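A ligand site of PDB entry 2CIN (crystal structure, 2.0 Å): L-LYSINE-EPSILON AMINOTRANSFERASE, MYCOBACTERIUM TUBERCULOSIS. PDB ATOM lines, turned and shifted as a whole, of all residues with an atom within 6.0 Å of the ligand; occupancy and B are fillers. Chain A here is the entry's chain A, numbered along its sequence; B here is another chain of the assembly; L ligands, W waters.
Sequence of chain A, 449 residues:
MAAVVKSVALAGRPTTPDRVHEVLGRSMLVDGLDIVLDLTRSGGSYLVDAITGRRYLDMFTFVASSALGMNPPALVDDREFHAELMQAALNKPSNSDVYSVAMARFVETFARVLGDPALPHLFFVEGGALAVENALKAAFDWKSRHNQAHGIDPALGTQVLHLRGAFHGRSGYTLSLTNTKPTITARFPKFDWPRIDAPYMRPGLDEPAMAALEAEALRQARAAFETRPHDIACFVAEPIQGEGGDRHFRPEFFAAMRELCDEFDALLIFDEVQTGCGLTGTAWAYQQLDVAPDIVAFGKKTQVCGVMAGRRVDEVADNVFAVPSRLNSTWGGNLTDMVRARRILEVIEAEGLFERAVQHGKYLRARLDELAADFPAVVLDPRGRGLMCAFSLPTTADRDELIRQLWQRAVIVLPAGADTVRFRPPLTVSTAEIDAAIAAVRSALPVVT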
ATOM      1  N   VAL A  63      17.761  33.916 -22.309  1.00  0.00           N
ATOM      2  CA  VAL A  63      18.868  32.947 -22.218  1.00  0.00           C
ATOM      3  C   VAL A  63      18.946  32.107 -23.498  1.00  0.00           C
ATOM      4  O   VAL A  63      18.945  30.876 -23.433  1.00  0.00           O
ATOM      5  CB  VAL A  63      18.773  32.031 -20.924  1.00  0.00           C
ATOM      6  CG1 VAL A  63      20.128  31.429 -20.574  1.00  0.00           C
ATOM      7  CG2 VAL A  63      18.168  32.828 -19.726  1.00  0.00           C
ATOM      8  N   GLY A 127      10.978  21.026 -20.651  1.00  0.00           N
ATOM      9  CA  GLY A 127      12.180  21.360 -19.881  1.00  0.00           C
ATOM     10  C   GLY A 127      13.436  20.731 -20.489  1.00  0.00           C
ATOM     11  O   GLY A 127      13.436  19.569 -20.881  1.00  0.00           O
ATOM     12  N   GLY A 128      14.505  21.535 -20.569  1.00  0.00           N
ATOM     13  CA  GLY A 128      15.756  21.084 -21.181  1.00  0.00           C
ATOM     14  C   GLY A 128      16.501  20.029 -20.363  1.00  0.00           C
ATOM     15  O   GLY A 128      17.091  19.093 -20.918  1.00  0.00           O
ATOM     16  N   ALA A 129      16.504  20.149 -19.037  1.00  0.00           N
ATOM     17  CA  ALA A 129      17.189  19.129 -18.210  1.00  0.00           C
ATOM     18  C   ALA A 129      16.512  17.746 -18.410  1.00  0.00           C
ATOM     19  O   ALA A 129      17.166  16.729 -18.518  1.00  0.00           O
ATOM     20  CB  ALA A 129      17.196  19.526 -16.753  1.00  0.00           C
ATOM     21  N   LEU A 130      15.196  17.729 -18.484  1.00  0.00           N
ATOM     22  CA  LEU A 130      14.480  16.483 -18.707  1.00  0.00           C
ATOM     23  C   LEU A 130      14.664  15.897 -20.131  1.00  0.00           C
ATOM     24  O   LEU A 130      14.640  14.683 -20.296  1.00  0.00           O
ATOM     25  CB  LEU A 130      13.003  16.650 -18.346  1.00  0.00           C
ATOM     26  CG  LEU A 130      12.569  15.916 -17.066  1.00  0.00           C
ATOM     27  CD1 LEU A 130      13.610  15.909 -15.955  1.00  0.00           C
ATOM     28  CD2 LEU A 130      11.241  16.408 -16.553  1.00  0.00           C
ATOM     29  N   VAL A 132      17.554  16.161 -21.691  1.00  0.00           N
ATOM     30  CA  VAL A 132      18.847  15.499 -21.488  1.00  0.00           C
ATOM     31  C   VAL A 132      18.652  14.219 -20.699  1.00  0.00           C
ATOM     32  O   VAL A 132      19.222  13.187 -21.053  1.00  0.00           O
ATOM     33  CB  VAL A 132      19.927  16.436 -20.802  1.00  0.00           C
ATOM     34  CG1 VAL A 132      21.206  15.650 -20.523  1.00  0.00           C
ATOM     35  CG2 VAL A 132      20.201  17.650 -21.709  1.00  0.00           C
ATOM     36  N   PHE A 167      27.507  22.013 -18.750  1.00  0.00           N
ATOM     37  CA  PHE A 167      26.235  22.369 -18.134  1.00  0.00           C
ATOM     38  C   PHE A 167      25.115  21.592 -18.851  1.00  0.00           C
ATOM     39  O   PHE A 167      24.891  21.812 -20.038  1.00  0.00           O
ATOM     40  CB  PHE A 167      25.955  23.863 -18.227  1.00  0.00           C
ATOM     41  CG  PHE A 167      24.685  24.264 -17.547  1.00  0.00           C
ATOM     42  CD1 PHE A 167      23.468  24.196 -18.226  1.00  0.00           C
ATOM     43  CD2 PHE A 167      24.690  24.640 -16.206  1.00  0.00           C
ATOM     44  CE1 PHE A 167      22.281  24.547 -17.566  1.00  0.00           C
ATOM     45  CE2 PHE A 167      23.505  24.975 -15.565  1.00  0.00           C
ATOM     46  CZ  PHE A 167      22.309  24.906 -16.236  1.00  0.00           C
ATOM     47  N   HIS A 168      24.430  20.724 -18.127  1.00  0.00           N
ATOM     48  CA  HIS A 168      23.382  19.892 -18.727  1.00  0.00           C
ATOM     49  C   HIS A 168      22.044  20.042 -17.982  1.00  0.00           C
ATOM     50  O   HIS A 168      21.060  19.405 -18.354  1.00  0.00           O
ATOM     51  CB  HIS A 168      23.833  18.437 -18.768  1.00  0.00           C
ATOM     52  CG  HIS A 168      25.018  18.208 -19.659  1.00  0.00           C
ATOM     53  ND1 HIS A 168      24.979  18.475 -21.008  1.00  0.00           N
ATOM     54  CD2 HIS A 168      26.277  17.787 -19.394  1.00  0.00           C
ATOM     55  CE1 HIS A 168      26.157  18.195 -21.547  1.00  0.00           C
ATOM     56  NE2 HIS A 168      26.968  17.801 -20.576  1.00  0.00           N
ATOM     57  N   GLY A 169      22.007  20.907 -16.980  1.00  0.00           N
ATOM     58  CA  GLY A 169      20.787  21.207 -16.254  1.00  0.00           C
ATOM     59  C   GLY A 169      20.905  20.969 -14.751  1.00  0.00           C
ATOM     60  O   GLY A 169      21.973  20.623 -14.240  1.00  0.00           O
ATOM     61  N   ARG A 170      19.767  21.116 -14.049  1.00  0.00           N
ATOM     62  CA  ARG A 170      19.733  21.126 -12.592  1.00  0.00           C
ATOM     63  C   ARG A 170      18.811  20.050 -11.982  1.00  0.00           C
ATOM     64  O   ARG A 170      18.344  20.166 -10.830  1.00  0.00           O
ATOM     65  CB  ARG A 170      19.289  22.521 -12.156  1.00  0.00           C
ATOM     66  CG  ARG A 170      20.334  23.622 -12.429  1.00  0.00           C
ATOM     67  CD  ARG A 170      19.656  24.927 -12.005  1.00  0.00           C
ATOM     68  NE  ARG A 170      20.437  26.128 -12.224  1.00  0.00           N
ATOM     69  CZ  ARG A 170      20.995  26.831 -11.246  1.00  0.00           C
ATOM     70  NH1 ARG A 170      20.912  26.422  -9.987  1.00  0.00           N
ATOM     71  NH2 ARG A 170      21.633  27.962 -11.521  1.00  0.00           N
ATOM     72  N   GLU A 238      28.136  19.037 -24.812  1.00  0.00           N
ATOM     73  CA  GLU A 238      27.711  20.168 -25.622  1.00  0.00           C
ATOM     74  C   GLU A 238      28.717  20.335 -26.776  1.00  0.00           C
ATOM     75  O   GLU A 238      29.919  20.297 -26.528  1.00  0.00           O
ATOM     76  CB  GLU A 238      27.762  21.434 -24.778  1.00  0.00           C
ATOM     77  CG  GLU A 238      26.823  21.389 -23.555  1.00  0.00           C
ATOM     78  CD  GLU A 238      27.324  22.347 -22.502  1.00  0.00           C
ATOM     79  OE1 GLU A 238      26.975  23.535 -22.596  1.00  0.00           O
ATOM     80  OE2 GLU A 238      28.099  21.900 -21.619  1.00  0.00           O
ATOM     81  N   GLY A 242      28.336  26.295 -23.439  1.00  0.00           N
ATOM     82  CA  GLY A 242      27.728  27.618 -23.295  1.00  0.00           C
ATOM     83  C   GLY A 242      27.977  28.234 -21.925  1.00  0.00           C
ATOM     84  O   GLY A 242      28.800  29.124 -21.816  1.00  0.00           O
ATOM     85  N   GLU A 243      27.275  27.752 -20.902  1.00  0.00           N
ATOM     86  CA  GLU A 243      27.409  28.290 -19.546  1.00  0.00           C
ATOM     87  C   GLU A 243      28.831  28.236 -19.008  1.00  0.00           C
ATOM     88  O   GLU A 243      29.234  29.106 -18.243  1.00  0.00           O
ATOM     89  CB  GLU A 243      26.470  27.590 -18.554  1.00  0.00           C
ATOM     90  CG  GLU A 243      25.022  27.571 -18.980  1.00  0.00           C
ATOM     91  CD  GLU A 243      24.447  28.969 -19.195  1.00  0.00           C
ATOM     92  OE1 GLU A 243      24.592  29.813 -18.293  1.00  0.00           O
ATOM     93  OE2 GLU A 243      23.819  29.223 -20.245  1.00  0.00           O
ATOM     94  N   ASP A 271      24.195  17.425 -26.400  1.00  0.00           N
ATOM     95  CA  ASP A 271      23.223  18.317 -25.757  1.00  0.00           C
ATOM     96  C   ASP A 271      23.255  19.603 -26.582  1.00  0.00           C
ATOM     97  O   ASP A 271      24.175  20.420 -26.440  1.00  0.00           O
ATOM     98  CB  ASP A 271      23.625  18.545 -24.283  1.00  0.00           C
ATOM     99  CG  ASP A 271      22.693  19.527 -23.536  1.00  0.00           C
ATOM    100  OD1 ASP A 271      21.833  20.169 -24.201  1.00  0.00           O
ATOM    101  OD2 ASP A 271      22.839  19.660 -22.294  1.00  0.00           O
ATOM    102  N   GLU A 272      22.293  19.711 -27.497  1.00  0.00           N
ATOM    103  CA  GLU A 272      22.100  20.892 -28.344  1.00  0.00           C
ATOM    104  C   GLU A 272      21.006  21.847 -27.825  1.00  0.00           C
ATOM    105  O   GLU A 272      20.451  22.622 -28.584  1.00  0.00           O
ATOM    106  CB  GLU A 272      21.775  20.475 -29.787  1.00  0.00           C
ATOM    107  CG  GLU A 272      22.955  19.747 -30.436  1.00  0.00           C
ATOM    108  CD  GLU A 272      23.597  20.497 -31.593  1.00  0.00           C
ATOM    109  OE1 GLU A 272      23.364  21.701 -31.828  1.00  0.00           O
ATOM    110  OE2 GLU A 272      24.342  19.817 -32.285  1.00  0.00           O
ATOM    111  N   VAL A 273      20.732  21.809 -26.536  1.00  0.00           N
ATOM    112  CA  VAL A 273      19.707  22.672 -25.959  1.00  0.00           C
ATOM    113  C   VAL A 273      20.049  24.144 -26.206  1.00  0.00           C
ATOM    114  O   VAL A 273      19.169  24.947 -26.581  1.00  0.00           O
ATOM    115  CB  VAL A 273      19.439  22.363 -24.427  1.00  0.00           C
ATOM    116  CG1 VAL A 273      18.529  23.456 -23.782  1.00  0.00           C
ATOM    117  CG2 VAL A 273      18.773  20.967 -24.258  1.00  0.00           C
ATOM    118  N   GLN A 274      21.324  24.492 -26.061  1.00  0.00           N
ATOM    119  CA  GLN A 274      21.753  25.866 -26.340  1.00  0.00           C
ATOM    120  C   GLN A 274      22.255  26.136 -27.771  1.00  0.00           C
ATOM    121  O   GLN A 274      22.079  27.250 -28.277  1.00  0.00           O
ATOM    122  CB  GLN A 274      22.775  26.324 -25.312  1.00  0.00           C
ATOM    123  CG  GLN A 274      22.877  27.866 -25.265  1.00  0.00           C
ATOM    124  CD  GLN A 274      23.677  28.412 -24.129  1.00  0.00           C
ATOM    125  OE1 GLN A 274      24.350  29.423 -24.289  1.00  0.00           O
ATOM    126  NE2 GLN A 274      23.584  27.783 -22.942  1.00  0.00           N
ATOM    127  N   THR A 275      22.894  25.150 -28.397  1.00  0.00           N
ATOM    128  CA  THR A 275      23.482  25.360 -29.727  1.00  0.00           C
ATOM    129  C   THR A 275      22.477  25.194 -30.875  1.00  0.00           C
ATOM    130  O   THR A 275      22.791  25.593 -32.025  1.00  0.00           O
ATOM    131  CB  THR A 275      24.691  24.382 -29.966  1.00  0.00           C
ATOM    132  OG1 THR A 275      24.246  23.054 -29.748  1.00  0.00           O
ATOM    133  CG2 THR A 275      25.833  24.681 -29.001  1.00  0.00           C
ATOM    134  N   LYS A 300      15.147  25.014 -25.258  1.00  0.00           N
ATOM    135  CA  LYS A 300      15.254  26.471 -25.402  1.00  0.00           C
ATOM    136  C   LYS A 300      14.491  26.981 -26.641  1.00  0.00           C
ATOM    137  O   LYS A 300      13.267  27.030 -26.624  1.00  0.00           O
ATOM    138  CB  LYS A 300      16.726  26.943 -25.273  1.00  0.00           C
ATOM    139  CG  LYS A 300      17.210  26.942 -23.807  1.00  0.00           C
ATOM    140  CD  LYS A 300      18.576  27.647 -23.574  1.00  0.00           C
ATOM    141  CE  LYS A 300      18.953  27.728 -22.059  1.00  0.00           C
ATOM    142  NZ  LYS A 300      19.809  26.511 -21.735  1.00  0.00           N
ATOM    143  N   CYS A 305      10.669  20.785 -25.417  1.00  0.00           N
ATOM    144  CA  CYS A 305      11.979  20.152 -25.397  1.00  0.00           C
ATOM    145  C   CYS A 305      11.874  18.675 -25.771  1.00  0.00           C
ATOM    146  O   CYS A 305      10.769  18.156 -25.960  1.00  0.00           O
ATOM    147  CB  CYS A 305      12.613  20.352 -24.016  1.00  0.00           C
ATOM    148  SG  CYS A 305      12.645  22.106 -23.578  1.00  0.00           S
ATOM    149  N   LEU B 130       9.857  17.559 -11.561  1.00  0.00           N
ATOM    150  CA  LEU B 130      10.795  18.616 -11.181  1.00  0.00           C
ATOM    151  C   LEU B 130      10.321  19.461  -9.962  1.00  0.00           C
ATOM    152  O   LEU B 130      11.150  19.940  -9.194  1.00  0.00           O
ATOM    153  CB  LEU B 130      11.132  19.487 -12.383  1.00  0.00           C
ATOM    154  CG  LEU B 130      12.565  19.310 -12.915  1.00  0.00           C
ATOM    155  CD1 LEU B 130      13.090  17.876 -12.855  1.00  0.00           C
ATOM    156  CD2 LEU B 130      12.732  19.873 -14.301  1.00  0.00           C
ATOM    157  N   ASN B 328      16.769  26.693  -9.957  1.00  0.00           N
ATOM    158  CA  ASN B 328      16.539  27.474 -11.194  1.00  0.00           C
ATOM    159  C   ASN B 328      16.094  26.561 -12.322  1.00  0.00           C
ATOM    160  O   ASN B 328      16.311  25.352 -12.271  1.00  0.00           O
ATOM    161  CB  ASN B 328      17.838  28.194 -11.630  1.00  0.00           C
ATOM    162  CG  ASN B 328      17.575  29.398 -12.589  1.00  0.00           C
ATOM    163  OD1 ASN B 328      16.709  30.244 -12.330  1.00  0.00           O
ATOM    164  ND2 ASN B 328      18.286  29.424 -13.731  1.00  0.00           N
ATOM    165  N   SER B 329      15.537  27.177 -13.349  1.00  0.00           N
ATOM    166  CA  SER B 329      15.386  26.568 -14.672  1.00  0.00           C
ATOM    167  C   SER B 329      15.415  27.756 -15.640  1.00  0.00           C
ATOM    168  O   SER B 329      15.223  28.924 -15.211  1.00  0.00           O
ATOM    169  CB  SER B 329      14.050  25.790 -14.778  1.00  0.00           C
ATOM    170  OG  SER B 329      12.914  26.645 -14.760  1.00  0.00           O
ATOM    171  N   THR B 330      15.649  27.491 -16.928  1.00  0.00           N
ATOM    172  CA  THR B 330      15.574  28.568 -17.940  1.00  0.00           C
ATOM    173  C   THR B 330      14.269  29.383 -17.861  1.00  0.00           C
ATOM    174  O   THR B 330      14.308  30.612 -17.751  1.00  0.00           O
ATOM    175  CB  THR B 330      15.783  28.026 -19.367  1.00  0.00           C
ATOM    176  OG1 THR B 330      17.055  27.356 -19.416  1.00  0.00           O
ATOM    177  CG2 THR B 330      15.736  29.136 -20.414  1.00  0.00           C
ATOM    178  N   TRP B 331      13.115  28.711 -17.916  1.00  0.00           N
ATOM    179  CA  TRP B 331      11.876  29.480 -18.038  1.00  0.00           C
ATOM    180  C   TRP B 331      11.205  29.901 -16.727  1.00  0.00           C
ATOM    181  O   TRP B 331      10.468  30.917 -16.723  1.00  0.00           O
ATOM    182  CB  TRP B 331      10.878  28.752 -18.939  1.00  0.00           C
ATOM    183  CG  TRP B 331      11.282  28.837 -20.405  1.00  0.00           C
ATOM    184  CD1 TRP B 331      11.473  29.963 -21.161  1.00  0.00           C
ATOM    185  CD2 TRP B 331      11.519  27.721 -21.295  1.00  0.00           C
ATOM    186  NE1 TRP B 331      11.812  29.628 -22.467  1.00  0.00           N
ATOM    187  CE2 TRP B 331      11.840  28.257 -22.570  1.00  0.00           C
ATOM    188  CE3 TRP B 331      11.456  26.324 -21.129  1.00  0.00           C
ATOM    189  CZ2 TRP B 331      12.125  27.431 -23.684  1.00  0.00           C
ATOM    190  CZ3 TRP B 331      11.749  25.500 -22.249  1.00  0.00           C
ATOM    191  CH2 TRP B 331      12.068  26.062 -23.502  1.00  0.00           C
HETATM  192  N1  LIG L   1      21.691  21.868 -21.424  1.00  0.00           N
HETATM  193  C1  LIG L   1      22.205  23.040 -21.938  1.00  0.00           C
HETATM  194  C2  LIG L   1      23.427  22.986 -22.849  1.00  0.00           C
HETATM  195  C3  LIG L   1      21.566  24.257 -21.639  1.00  0.00           C
HETATM  196  O1  LIG L   1      21.974  25.386 -22.297  1.00  0.00           O
HETATM  197  C4  LIG L   1      20.404  24.305 -20.803  1.00  0.00           C
HETATM  198  C5  LIG L   1      19.452  25.509 -20.992  1.00  0.00           C
HETATM  199  C6  LIG L   1      19.920  23.092 -20.284  1.00  0.00           C
HETATM  200  C7  LIG L   1      20.560  21.879 -20.597  1.00  0.00           C
HETATM  201  C8  LIG L   1      18.845  23.030 -19.198  1.00  0.00           C
HETATM  202  O2  LIG L   1      17.617  23.433 -19.782  1.00  0.00           O
HETATM  203  P1  LIG L   1      16.437  23.946 -18.787  1.00  0.00           P
HETATM  204  O3  LIG L   1      16.308  22.842 -17.777  1.00  0.00           O
HETATM  205  O4  LIG L   1      16.868  25.180 -18.014  1.00  0.00           O
HETATM  206  O5  LIG L   1      15.201  24.190 -19.633  1.00  0.00           O
HETATM  207  O   HOH W   1      25.368  25.538 -21.564  1.00  0.00           O
HETATM  208  O   HOH W   2      17.749  22.682 -15.599  1.00  0.00           O
HETATM  209  O   HOH W   3      13.417  25.708 -18.313  1.00  0.00           O
HETATM  210  O   HOH W   4      14.975  24.686 -22.275  1.00  0.00           O
HETATM  211  O   HOH W   5      23.853  23.116 -26.262  1.00  0.00           O
HETATM  212  O   HOH W   6      14.147  22.325 -16.249  1.00  0.00           O
HETATM  213  O   HOH W   7      18.652  25.290 -15.887  1.00  0.00           O
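O of Phe 167 sits close to N1 of the ligand, 3.5 Å away. Residues that only touch the ligand: His 168 (3.4 Å), Val 273 (3.6 Å), Glu 238 (3.6 Å), Ser 329 of chain B (3.8 Å), Gly 169 (3.97 Å) and Gly 127 (3.98 Å). Hydrophobic or aromatic side chains that line the ligand: Ala 129, Phe 167 and Val 273. Of the 25 residues printed, 13 come within 4 Å of the ligand. The nearest printed residue that does not touch the ligand is Val 132 (4.4 Å).
Water W2 bridges O3 of the ligand (2.6 Å) and N of Arg 170 (3.0 Å). Water W3 lies within hydrogen-bond range of O5 of the ligand (2.7 Å), N of Trp 331 of chain B (3.0 Å) and N of Thr 330 of chain B (3.2 Å). Water W4 lies within hydrogen-bond range of O5 of the ligand (2.7 Å), N of Lys 300 (3.0 Å) and SG of Cys 305 (3.7 Å). Water W1 lies within hydrogen-bond range of the side-chain carboxylate of Glu 238, the backbone NH of Glu 243, the side-chain amide nitrogen of Gln 274 and an oxygen (O1) of the ligand.
The side-chain carboxylate (OD2) of Asp 271 lies within hydrogen-bond range of a ring nitrogen (ND1) of His 168 (2.8 Å). The backbone NH of Gly 127 lies close to the side-chain sulfur of Cys 305 (3.5 Å). The backbone NH of Phe 167 sits at hydrogen-bond distance from the side-chain carboxylate of Glu 238 (2.9 Å). N of Gly 242 is in hydrogen-bond range of OE1 of Glu 238, at 3.2 Å. The side-chain carboxylate (OE2) of Glu 243 sits at hydrogen-bond distance from the side-chain amide nitrogen (NE2) of Gln 274 (3.1 Å). The backbone NH (N) of Gly 128 is in hydrogen-bond range of the side-chain sulfur (SG) of Cys 305. OD1 of Asp 271 is in hydrogen-bond range of N of Val 273 (3.1 Å).
A nitrogen (N1) of the ligand lies within hydrogen-bond range of the side-chain carboxylate (OD2) of Asp 271, at 2.6 Å. N of Gly 128 lies within hydrogen-bond range of O5 of the ligand. O3 of the ligand sits at hydrogen-bond distance from N of Ala 129 (3.0 Å). The side-chain hydroxyl (OG1) of Thr 330 of chain B sits at hydrogen-bond distance from an oxygen (O4) of the ligand (2.6 Å). An oxygen (O1) of the ligand is in hydrogen-bond range of the side-chain amide nitrogen (NE2) of Gln 274, 3.0 Å away. NZ of Lys 300 is bonded to C5 of the ligand (1.3 Å). N of Thr 330 of chain B lies within hydrogen-bond range of O4 of the ligand (2.8 Å).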
